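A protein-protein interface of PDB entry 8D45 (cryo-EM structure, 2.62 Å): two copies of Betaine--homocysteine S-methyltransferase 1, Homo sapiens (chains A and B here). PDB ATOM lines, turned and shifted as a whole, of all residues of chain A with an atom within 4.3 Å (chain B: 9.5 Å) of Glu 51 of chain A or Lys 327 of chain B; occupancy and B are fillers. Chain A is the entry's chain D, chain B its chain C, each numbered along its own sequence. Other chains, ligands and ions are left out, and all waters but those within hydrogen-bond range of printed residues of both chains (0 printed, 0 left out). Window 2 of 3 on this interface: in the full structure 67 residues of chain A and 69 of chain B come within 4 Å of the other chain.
The side-chain hydroxyl (OH) of Tyr 38 of chain A sits at hydrogen-bond distance from the side-chain amide oxygen (OE1) of Gln 58 of chain B (2.7 Å). NH2 of Arg 65 of chain B lies within hydrogen-bond range of O of Gly 37 of chain A (3.0 Å). NE2 of His 52 of chain A lies within hydrogen-bond range of NH1 of Arg 65 of chain B (3.5 Å). NZ of Lys 327 of chain B lies within salt-bridge range of OE1 of Glu 51 of chain A, 3.4 Å away.
O of Arg 65 of chain B is in hydrogen-bond range of N of Ala 324 of chain B, 3.0 Å away. The guanidinium group of Arg 65 of chain B is in salt-bridge range of the side-chain carboxylate of Glu 326 of chain B. NH1 of Arg 278 of chain B lies within hydrogen-bond range of NE2 of His 328 of chain B (3.2 Å). The guanidinium group (NE) of Arg 308 of chain B lies within salt-bridge range of the side-chain carboxylate (OE2) of Glu 312 of chain B (3.9 Å). The guanidinium group (NE) of Arg 308 of chain B is in hydrogen-bond range of a ring nitrogen (ND1) of His 328 of chain B. ND1 of His 328 of chain B lies within hydrogen-bond range of OE2 of Glu 312 of chain B (2.8 Å).
CA of Gly 37 of chain A touches NH1 of Arg 308 of chain B, 3.7 Å away. Lys 327 of chain B touches Gly 37 of chain A. Arg 65 of chain B touches Tyr 38 of chain A (CD to CE1, 3.5 Å). O of Tyr 38 of chain A touches CE of Lys 327 of chain B, 3.6 Å away. O of Val 39 of chain A touches O of Lys 327 of chain B, at 3.6 Å. CD of Lys 40 of chain A touches O of Glu 326 of chain B, at 3.9 Å. Lys 327 of chain B touches Lys 40 of chain A. Lys 40 of chain A touches His 328 of chain B. Gly 334 of chain B touches Lys 40 of chain A (CA to CE, 3.9 Å).
Of the printed residues of chain B, Gly 37 of chain A touches Arg 65, Arg 308 and Lys 327. Of the printed residues of chain B, Lys 40 of chain A touches Glu 326, Lys 327, His 328 and Gly 334. Of chain B, only Lys 327 comes within 4 Å of Glu 51 of chain A. Printed residues of chain A within 4 Å of Arg 65 of chain B: Gly 37 (3.0 Å), Tyr 38 (3.5 Å) and His 52 (3.5 Å). Of the printed residues of chain A, Glu 326 of chain B touches Lys 40. Lys 327 of chain B touches just these residues of chain A: Gly 37 (3.2 Å), Tyr 38 (3.6 Å), Val 39 (3.6 Å), Lys 40 (3.8 Å) and Glu 51 (3.4 Å). Printed residues of chain A within 4 Å of Gly 334 of chain B: Lys 40 (3.9 Å). The nearest printed residue of chain A that does not touch His 328 of chain B is Val 39 of chain A (5.5 Å).
Of the 11 printed residues of chain A, 6 touch a printed residue of chain B. Along chain A the printed residues that touch a printed residue of chain B span positions 37 to 52. Among the printed residues, 13 pairs touch across the chains.
No position is printed for both chains.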
ATOM      1  N   GLY A  37     -17.660 -27.215 -20.647  1.00  0.00           N
ATOM      2  CA  GLY A  37     -16.460 -26.834 -21.359  1.00  0.00           C
ATOM      3  C   GLY A  37     -15.165 -27.377 -20.805  1.00  0.00           C
ATOM      4  O   GLY A  37     -14.096 -26.963 -21.271  1.00  0.00           O
ATOM      5  N   TYR A  38     -15.216 -28.293 -19.837  1.00  0.00           N
ATOM      6  CA  TYR A  38     -14.007 -28.755 -19.164  1.00  0.00           C
ATOM      7  C   TYR A  38     -13.606 -30.170 -19.553  1.00  0.00           C
ATOM      8  O   TYR A  38     -12.443 -30.545 -19.366  1.00  0.00           O
ATOM      9  CB  TYR A  38     -14.200 -28.657 -17.651  1.00  0.00           C
ATOM     10  CG  TYR A  38     -14.435 -27.236 -17.207  1.00  0.00           C
ATOM     11  CD1 TYR A  38     -13.434 -26.283 -17.319  1.00  0.00           C
ATOM     12  CD2 TYR A  38     -15.661 -26.839 -16.703  1.00  0.00           C
ATOM     13  CE1 TYR A  38     -13.642 -24.981 -16.930  1.00  0.00           C
ATOM     14  CE2 TYR A  38     -15.880 -25.535 -16.310  1.00  0.00           C
ATOM     15  CZ  TYR A  38     -14.866 -24.611 -16.426  1.00  0.00           C
ATOM     16  OH  TYR A  38     -15.072 -23.312 -16.035  1.00  0.00           O
ATOM     17  N   VAL A  39     -14.529 -30.960 -20.089  1.00  0.00           N
ATOM     18  CA  VAL A  39     -14.225 -32.276 -20.638  1.00  0.00           C
ATOM     19  C   VAL A  39     -14.530 -32.247 -22.127  1.00  0.00           C
ATOM     20  O   VAL A  39     -15.415 -31.517 -22.584  1.00  0.00           O
ATOM     21  CB  VAL A  39     -15.021 -33.397 -19.934  1.00  0.00           C
ATOM     22  CG1 VAL A  39     -14.776 -34.733 -20.610  1.00  0.00           C
ATOM     23  CG2 VAL A  39     -14.636 -33.483 -18.470  1.00  0.00           C
ATOM     24  N   LYS A  40     -13.775 -33.030 -22.889  1.00  0.00           N
ATOM     25  CA  LYS A  40     -14.006 -33.178 -24.318  1.00  0.00           C
ATOM     26  C   LYS A  40     -14.805 -34.447 -24.587  1.00  0.00           C
ATOM     27  O   LYS A  40     -14.667 -35.452 -23.888  1.00  0.00           O
ATOM     28  CB  LYS A  40     -12.689 -33.222 -25.096  1.00  0.00           C
ATOM     29  CG  LYS A  40     -12.881 -33.131 -26.600  1.00  0.00           C
ATOM     30  CD  LYS A  40     -11.584 -32.833 -27.330  1.00  0.00           C
ATOM     31  CE  LYS A  40     -11.662 -33.284 -28.780  1.00  0.00           C
ATOM     32  NZ  LYS A  40     -10.444 -32.936 -29.557  1.00  0.00           N
ATOM     33  N   GLU A  47      -8.947 -34.352 -17.717  1.00  0.00           N
ATOM     34  CA  GLU A  47      -7.826 -33.420 -17.640  1.00  0.00           C
ATOM     35  C   GLU A  47      -8.179 -32.143 -16.887  1.00  0.00           C
ATOM     36  O   GLU A  47      -7.284 -31.339 -16.607  1.00  0.00           O
ATOM     37  CB  GLU A  47      -7.328 -33.069 -19.045  1.00  0.00           C
ATOM     38  CG  GLU A  47      -7.082 -34.267 -19.953  1.00  0.00           C
ATOM     39  CD  GLU A  47      -5.844 -35.053 -19.559  1.00  0.00           C
ATOM     40  OE1 GLU A  47      -5.265 -34.760 -18.492  1.00  0.00           O
ATOM     41  OE2 GLU A  47      -5.447 -35.962 -20.317  1.00  0.00           O
ATOM     42  N   ALA A  48      -9.454 -31.935 -16.554  1.00  0.00           N
ATOM     43  CA  ALA A  48      -9.876 -30.723 -15.861  1.00  0.00           C
ATOM     44  C   ALA A  48      -9.639 -30.773 -14.358  1.00  0.00           C
ATOM     45  O   ALA A  48      -9.818 -29.747 -13.697  1.00  0.00           O
ATOM     46  CB  ALA A  48     -11.359 -30.461 -16.124  1.00  0.00           C
ATOM     47  N   ALA A  49      -9.253 -31.922 -13.802  1.00  0.00           N
ATOM     48  CA  ALA A  49      -9.089 -32.016 -12.354  1.00  0.00           C
ATOM     49  C   ALA A  49      -7.917 -31.170 -11.873  1.00  0.00           C
ATOM     50  O   ALA A  49      -7.970 -30.591 -10.782  1.00  0.00           O
ATOM     51  CB  ALA A  49      -8.903 -33.475 -11.941  1.00  0.00           C
ATOM     52  N   VAL A  50      -6.850 -31.092 -12.668  1.00  0.00           N
ATOM     53  CA  VAL A  50      -5.673 -30.309 -12.309  1.00  0.00           C
ATOM     54  C   VAL A  50      -5.725 -28.975 -13.040  1.00  0.00           C
ATOM     55  O   VAL A  50      -5.275 -27.949 -12.515  1.00  0.00           O
ATOM     56  CB  VAL A  50      -4.367 -31.063 -12.632  1.00  0.00           C
ATOM     57  CG1 VAL A  50      -4.283 -32.349 -11.829  1.00  0.00           C
ATOM     58  CG2 VAL A  50      -4.247 -31.347 -14.128  1.00  0.00           C
ATOM     59  N   GLU A  51      -6.274 -28.977 -14.256  1.00  0.00           N
ATOM     60  CA  GLU A  51      -6.360 -27.745 -15.029  1.00  0.00           C
ATOM     61  C   GLU A  51      -7.384 -26.781 -14.442  1.00  0.00           C
ATOM     62  O   GLU A  51      -7.118 -25.578 -14.344  1.00  0.00           O
ATOM     63  CB  GLU A  51      -6.704 -28.060 -16.484  1.00  0.00           C
ATOM     64  CG  GLU A  51      -5.557 -28.673 -17.266  1.00  0.00           C
ATOM     65  CD  GLU A  51      -6.001 -29.273 -18.584  1.00  0.00           C
ATOM     66  OE1 GLU A  51      -6.915 -28.707 -19.218  1.00  0.00           O
ATOM     67  OE2 GLU A  51      -5.433 -30.309 -18.986  1.00  0.00           O
ATOM     68  N   HIS A  52      -8.551 -27.284 -14.043  1.00  0.00           N
ATOM     69  CA  HIS A  52      -9.650 -26.445 -13.565  1.00  0.00           C
ATOM     70  C   HIS A  52     -10.208 -27.029 -12.276  1.00  0.00           C
ATOM     71  O   HIS A  52     -11.338 -27.526 -12.235  1.00  0.00           O
ATOM     72  CB  HIS A  52     -10.736 -26.327 -14.636  1.00  0.00           C
ATOM     73  CG  HIS A  52     -10.280 -25.618 -15.873  1.00  0.00           C
ATOM     74  ND1 HIS A  52      -9.889 -26.289 -17.012  1.00  0.00           N
ATOM     75  CD2 HIS A  52     -10.138 -24.300 -16.144  1.00  0.00           C
ATOM     76  CE1 HIS A  52      -9.531 -25.415 -17.935  1.00  0.00           C
ATOM     77  NE2 HIS A  52      -9.672 -24.200 -17.433  1.00  0.00           N
ATOM     78  N   PRO A  53      -9.432 -26.980 -11.191  1.00  0.00           N
ATOM     79  CA  PRO A  53      -9.942 -27.479  -9.905  1.00  0.00           C
ATOM     80  C   PRO A  53     -11.200 -26.778  -9.425  1.00  0.00           C
ATOM     81  O   PRO A  53     -12.025 -27.415  -8.762  1.00  0.00           O
ATOM     82  CB  PRO A  53      -8.767 -27.238  -8.944  1.00  0.00           C
ATOM     83  CG  PRO A  53      -7.805 -26.363  -9.693  1.00  0.00           C
ATOM     84  CD  PRO A  53      -7.992 -26.698 -11.122  1.00  0.00           C
ATOM     85  N   GLN B  58     -18.417 -19.144 -10.866  1.00  0.00           N
ATOM     86  CA  GLN B  58     -18.062 -20.249 -11.746  1.00  0.00           C
ATOM     87  C   GLN B  58     -18.939 -20.268 -12.990  1.00  0.00           C
ATOM     88  O   GLN B  58     -18.460 -20.591 -14.079  1.00  0.00           O
ATOM     89  CB  GLN B  58     -18.158 -21.572 -10.981  1.00  0.00           C
ATOM     90  CG  GLN B  58     -17.782 -22.816 -11.782  1.00  0.00           C
ATOM     91  CD  GLN B  58     -16.428 -22.713 -12.458  1.00  0.00           C
ATOM     92  OE1 GLN B  58     -16.273 -23.102 -13.614  1.00  0.00           O
ATOM     93  NE2 GLN B  58     -15.445 -22.181 -11.747  1.00  0.00           N
ATOM     94  N   ARG B  61     -17.473 -17.660 -15.205  1.00  0.00           N
ATOM     95  CA  ARG B  61     -16.247 -18.151 -15.820  1.00  0.00           C
ATOM     96  C   ARG B  61     -16.498 -19.210 -16.883  1.00  0.00           C
ATOM     97  O   ARG B  61     -15.780 -19.242 -17.883  1.00  0.00           O
ATOM     98  CB  ARG B  61     -15.312 -18.720 -14.753  1.00  0.00           C
ATOM     99  CG  ARG B  61     -13.851 -18.373 -14.965  1.00  0.00           C
ATOM    100  CD  ARG B  61     -13.036 -18.640 -13.715  1.00  0.00           C
ATOM    101  NE  ARG B  61     -13.236 -17.619 -12.695  1.00  0.00           N
ATOM    102  CZ  ARG B  61     -12.736 -17.676 -11.467  1.00  0.00           C
ATOM    103  NH1 ARG B  61     -12.012 -18.705 -11.060  1.00  0.00           N
ATOM    104  NH2 ARG B  61     -12.967 -16.674 -10.626  1.00  0.00           N
ATOM    105  N   ARG B  65     -15.420 -18.751 -20.671  1.00  0.00           N
ATOM    106  CA  ARG B  65     -14.686 -19.796 -21.374  1.00  0.00           C
ATOM    107  C   ARG B  65     -15.393 -20.188 -22.663  1.00  0.00           C
ATOM    108  O   ARG B  65     -14.742 -20.459 -23.679  1.00  0.00           O
ATOM    109  CB  ARG B  65     -14.533 -21.004 -20.453  1.00  0.00           C
ATOM    110  CG  ARG B  65     -13.439 -21.974 -20.840  1.00  0.00           C
ATOM    111  CD  ARG B  65     -13.342 -23.100 -19.825  1.00  0.00           C
ATOM    112  NE  ARG B  65     -12.896 -24.347 -20.431  1.00  0.00           N
ATOM    113  CZ  ARG B  65     -11.657 -24.587 -20.834  1.00  0.00           C
ATOM    114  NH1 ARG B  65     -10.699 -23.683 -20.705  1.00  0.00           N
ATOM    115  NH2 ARG B  65     -11.370 -25.763 -21.381  1.00  0.00           N
ATOM    116  N   ARG B 278     -26.262 -28.226 -29.816  1.00  0.00           N
ATOM    117  CA  ARG B 278     -25.170 -27.370 -30.249  1.00  0.00           C
ATOM    118  C   ARG B 278     -25.155 -27.169 -31.756  1.00  0.00           C
ATOM    119  O   ARG B 278     -24.370 -26.356 -32.248  1.00  0.00           O
ATOM    120  CB  ARG B 278     -23.838 -27.950 -29.780  1.00  0.00           C
ATOM    121  CG  ARG B 278     -23.455 -29.261 -30.434  1.00  0.00           C
ATOM    122  CD  ARG B 278     -22.333 -29.941 -29.677  1.00  0.00           C
ATOM    123  NE  ARG B 278     -22.702 -30.190 -28.289  1.00  0.00           N
ATOM    124  CZ  ARG B 278     -21.842 -30.360 -27.297  1.00  0.00           C
ATOM    125  NH1 ARG B 278     -20.537 -30.285 -27.492  1.00  0.00           N
ATOM    126  NH2 ARG B 278     -22.303 -30.608 -26.075  1.00  0.00           N
ATOM    127  N   TYR B 305     -22.188 -24.500 -23.324  1.00  0.00           N
ATOM    128  CA  TYR B 305     -21.890 -25.179 -24.581  1.00  0.00           C
ATOM    129  C   TYR B 305     -22.696 -24.599 -25.739  1.00  0.00           C
ATOM    130  O   TYR B 305     -22.235 -24.625 -26.883  1.00  0.00           O
ATOM    131  CB  TYR B 305     -22.112 -26.690 -24.427  1.00  0.00           C
ATOM    132  CG  TYR B 305     -23.551 -27.151 -24.431  1.00  0.00           C
ATOM    133  CD1 TYR B 305     -24.329 -27.057 -23.290  1.00  0.00           C
ATOM    134  CD2 TYR B 305     -24.120 -27.710 -25.564  1.00  0.00           C
ATOM    135  CE1 TYR B 305     -25.633 -27.475 -23.283  1.00  0.00           C
ATOM    136  CE2 TYR B 305     -25.425 -28.139 -25.563  1.00  0.00           C
ATOM    137  CZ  TYR B 305     -26.177 -28.017 -24.419  1.00  0.00           C
ATOM    138  OH  TYR B 305     -27.482 -28.442 -24.405  1.00  0.00           O
ATOM    139  N   ARG B 308     -20.618 -21.675 -26.620  1.00  0.00           N
ATOM    140  CA  ARG B 308     -19.483 -22.197 -27.366  1.00  0.00           C
ATOM    141  C   ARG B 308     -19.869 -22.564 -28.789  1.00  0.00           C
ATOM    142  O   ARG B 308     -19.047 -22.420 -29.694  1.00  0.00           O
ATOM    143  CB  ARG B 308     -18.886 -23.411 -26.657  1.00  0.00           C
ATOM    144  CG  ARG B 308     -17.733 -24.047 -27.420  1.00  0.00           C
ATOM    145  CD  ARG B 308     -16.982 -25.068 -26.586  1.00  0.00           C
ATOM    146  NE  ARG B 308     -17.701 -26.330 -26.450  1.00  0.00           N
ATOM    147  CZ  ARG B 308     -18.374 -26.718 -25.373  1.00  0.00           C
ATOM    148  NH1 ARG B 308     -18.468 -25.956 -24.295  1.00  0.00           N
ATOM    149  NH2 ARG B 308     -18.975 -27.904 -25.380  1.00  0.00           N
ATOM    150  N   GLU B 312     -17.983 -21.017 -31.922  1.00  0.00           N
ATOM    151  CA  GLU B 312     -17.341 -21.881 -32.902  1.00  0.00           C
ATOM    152  C   GLU B 312     -17.927 -21.677 -34.291  1.00  0.00           C
ATOM    153  O   GLU B 312     -17.202 -21.751 -35.289  1.00  0.00           O
ATOM    154  CB  GLU B 312     -17.471 -23.340 -32.472  1.00  0.00           C
ATOM    155  CG  GLU B 312     -16.458 -23.752 -31.422  1.00  0.00           C
ATOM    156  CD  GLU B 312     -16.437 -25.244 -31.172  1.00  0.00           C
ATOM    157  OE1 GLU B 312     -16.527 -26.013 -32.150  1.00  0.00           O
ATOM    158  OE2 GLU B 312     -16.324 -25.647 -29.997  1.00  0.00           O
ATOM    159  N   LEU B 321     -10.987 -18.837 -32.065  1.00  0.00           N
ATOM    160  CA  LEU B 321     -11.912 -19.741 -31.407  1.00  0.00           C
ATOM    161  C   LEU B 321     -11.883 -19.499 -29.904  1.00  0.00           C
ATOM    162  O   LEU B 321     -10.858 -19.077 -29.355  1.00  0.00           O
ATOM    163  CB  LEU B 321     -11.558 -21.204 -31.704  1.00  0.00           C
ATOM    164  CG  LEU B 321     -11.917 -21.687 -33.110  1.00  0.00           C
ATOM    165  CD1 LEU B 321     -10.665 -21.941 -33.934  1.00  0.00           C
ATOM    166  CD2 LEU B 321     -12.781 -22.933 -33.043  1.00  0.00           C
ATOM    167  N   PRO B 322     -12.984 -19.756 -29.204  1.00  0.00           N
ATOM    168  CA  PRO B 322     -13.028 -19.484 -27.769  1.00  0.00           C
ATOM    169  C   PRO B 322     -12.096 -20.411 -27.010  1.00  0.00           C
ATOM    170  O   PRO B 322     -11.565 -21.374 -27.581  1.00  0.00           O
ATOM    171  CB  PRO B 322     -14.496 -19.750 -27.412  1.00  0.00           C
ATOM    172  CG  PRO B 322     -14.915 -20.765 -28.407  1.00  0.00           C
ATOM    173  CD  PRO B 322     -14.256 -20.325 -29.679  1.00  0.00           C
ATOM    174  N   PRO B 323     -11.850 -20.141 -25.725  1.00  0.00           N
ATOM    175  CA  PRO B 323     -11.023 -21.076 -24.940  1.00  0.00           C
ATOM    176  C   PRO B 323     -11.592 -22.483 -24.899  1.00  0.00           C
ATOM    177  O   PRO B 323     -10.864 -23.456 -25.137  1.00  0.00           O
ATOM    178  CB  PRO B 323     -10.999 -20.438 -23.544  1.00  0.00           C
ATOM    179  CG  PRO B 323     -11.334 -19.009 -23.745  1.00  0.00           C
ATOM    180  CD  PRO B 323     -12.146 -18.895 -24.997  1.00  0.00           C
ATOM    181  N   ALA B 324     -12.895 -22.615 -24.645  1.00  0.00           N
ATOM    182  CA  ALA B 324     -13.510 -23.923 -24.459  1.00  0.00           C
ATOM    183  C   ALA B 324     -13.456 -24.782 -25.708  1.00  0.00           C
ATOM    184  O   ALA B 324     -13.693 -25.991 -25.613  1.00  0.00           O
ATOM    185  CB  ALA B 324     -14.962 -23.761 -24.006  1.00  0.00           C
ATOM    186  N   SER B 325     -13.134 -24.209 -26.868  1.00  0.00           N
ATOM    187  CA  SER B 325     -12.926 -25.023 -28.055  1.00  0.00           C
ATOM    188  C   SER B 325     -11.793 -26.020 -27.877  1.00  0.00           C
ATOM    189  O   SER B 325     -11.707 -26.974 -28.656  1.00  0.00           O
ATOM    190  CB  SER B 325     -12.647 -24.141 -29.268  1.00  0.00           C
ATOM    191  OG  SER B 325     -13.799 -23.403 -29.625  1.00  0.00           O
ATOM    192  N   GLU B 326     -10.919 -25.826 -26.886  1.00  0.00           N
ATOM    193  CA  GLU B 326      -9.922 -26.852 -26.611  1.00  0.00           C
ATOM    194  C   GLU B 326     -10.587 -28.155 -26.189  1.00  0.00           C
ATOM    195  O   GLU B 326     -10.136 -29.235 -26.585  1.00  0.00           O
ATOM    196  CB  GLU B 326      -8.935 -26.371 -25.545  1.00  0.00           C
ATOM    197  CG  GLU B 326      -9.513 -26.232 -24.152  1.00  0.00           C
ATOM    198  CD  GLU B 326      -8.639 -25.385 -23.246  1.00  0.00           C
ATOM    199  OE1 GLU B 326      -8.813 -24.148 -23.231  1.00  0.00           O
ATOM    200  OE2 GLU B 326      -7.776 -25.958 -22.548  1.00  0.00           O
ATOM    201  N   LYS B 327     -11.657 -28.078 -25.406  1.00  0.00           N
ATOM    202  CA  LYS B 327     -12.438 -29.254 -25.013  1.00  0.00           C
ATOM    203  C   LYS B 327     -13.607 -29.477 -25.965  1.00  0.00           C
ATOM    204  O   LYS B 327     -14.747 -29.666 -25.542  1.00  0.00           O
ATOM    205  CB  LYS B 327     -12.930 -29.094 -23.579  1.00  0.00           C
ATOM    206  CG  LYS B 327     -11.833 -28.859 -22.546  1.00  0.00           C
ATOM    207  CD  LYS B 327     -10.760 -29.939 -22.587  1.00  0.00           C
ATOM    208  CE  LYS B 327      -9.690 -29.704 -21.539  1.00  0.00           C
ATOM    209  NZ  LYS B 327      -8.327 -29.947 -22.085  1.00  0.00           N
ATOM    210  N   HIS B 328     -13.333 -29.467 -27.268  1.00  0.00           N
ATOM    211  CA  HIS B 328     -14.357 -29.704 -28.276  1.00  0.00           C
ATOM    212  C   HIS B 328     -13.708 -29.777 -29.648  1.00  0.00           C
ATOM    213  O   HIS B 328     -12.697 -29.115 -29.896  1.00  0.00           O
ATOM    214  CB  HIS B 328     -15.425 -28.599 -28.274  1.00  0.00           C
ATOM    215  CG  HIS B 328     -16.708 -28.998 -28.936  1.00  0.00           C
ATOM    216  ND1 HIS B 328     -17.634 -28.077 -29.376  1.00  0.00           N
ATOM    217  CD2 HIS B 328     -17.218 -30.215 -29.238  1.00  0.00           C
ATOM    218  CE1 HIS B 328     -18.657 -28.709 -29.921  1.00  0.00           C
ATOM    219  NE2 HIS B 328     -18.430 -30.008 -29.849  1.00  0.00           N
ATOM    220  N   GLY B 329     -14.297 -30.578 -30.529  1.00  0.00           N
ATOM    221  CA  GLY B 329     -13.950 -30.562 -31.933  1.00  0.00           C
ATOM    222  C   GLY B 329     -14.818 -29.575 -32.685  1.00  0.00           C
ATOM    223  O   GLY B 329     -15.569 -28.790 -32.101  1.00  0.00           O
ATOM    224  N   SER B 330     -14.713 -29.621 -34.011  1.00  0.00           N
ATOM    225  CA  SER B 330     -15.521 -28.788 -34.893  1.00  0.00           C
ATOM    226  C   SER B 330     -16.490 -29.691 -35.638  1.00  0.00           C
ATOM    227  O   SER B 330     -16.069 -30.525 -36.445  1.00  0.00           O
ATOM    228  CB  SER B 330     -14.648 -28.003 -35.876  1.00  0.00           C
ATOM    229  OG  SER B 330     -15.418 -27.521 -36.963  1.00  0.00           O
ATOM    230  N   GLY B 334     -14.143 -34.442 -32.851  1.00  0.00           N
ATOM    231  CA  GLY B 334     -13.394 -35.096 -31.793  1.00  0.00           C
ATOM    232  C   GLY B 334     -13.668 -36.578 -31.645  1.00  0.00           C
ATOM    233  O   GLY B 334     -12.926 -37.251 -30.921  1.00  0.00           O
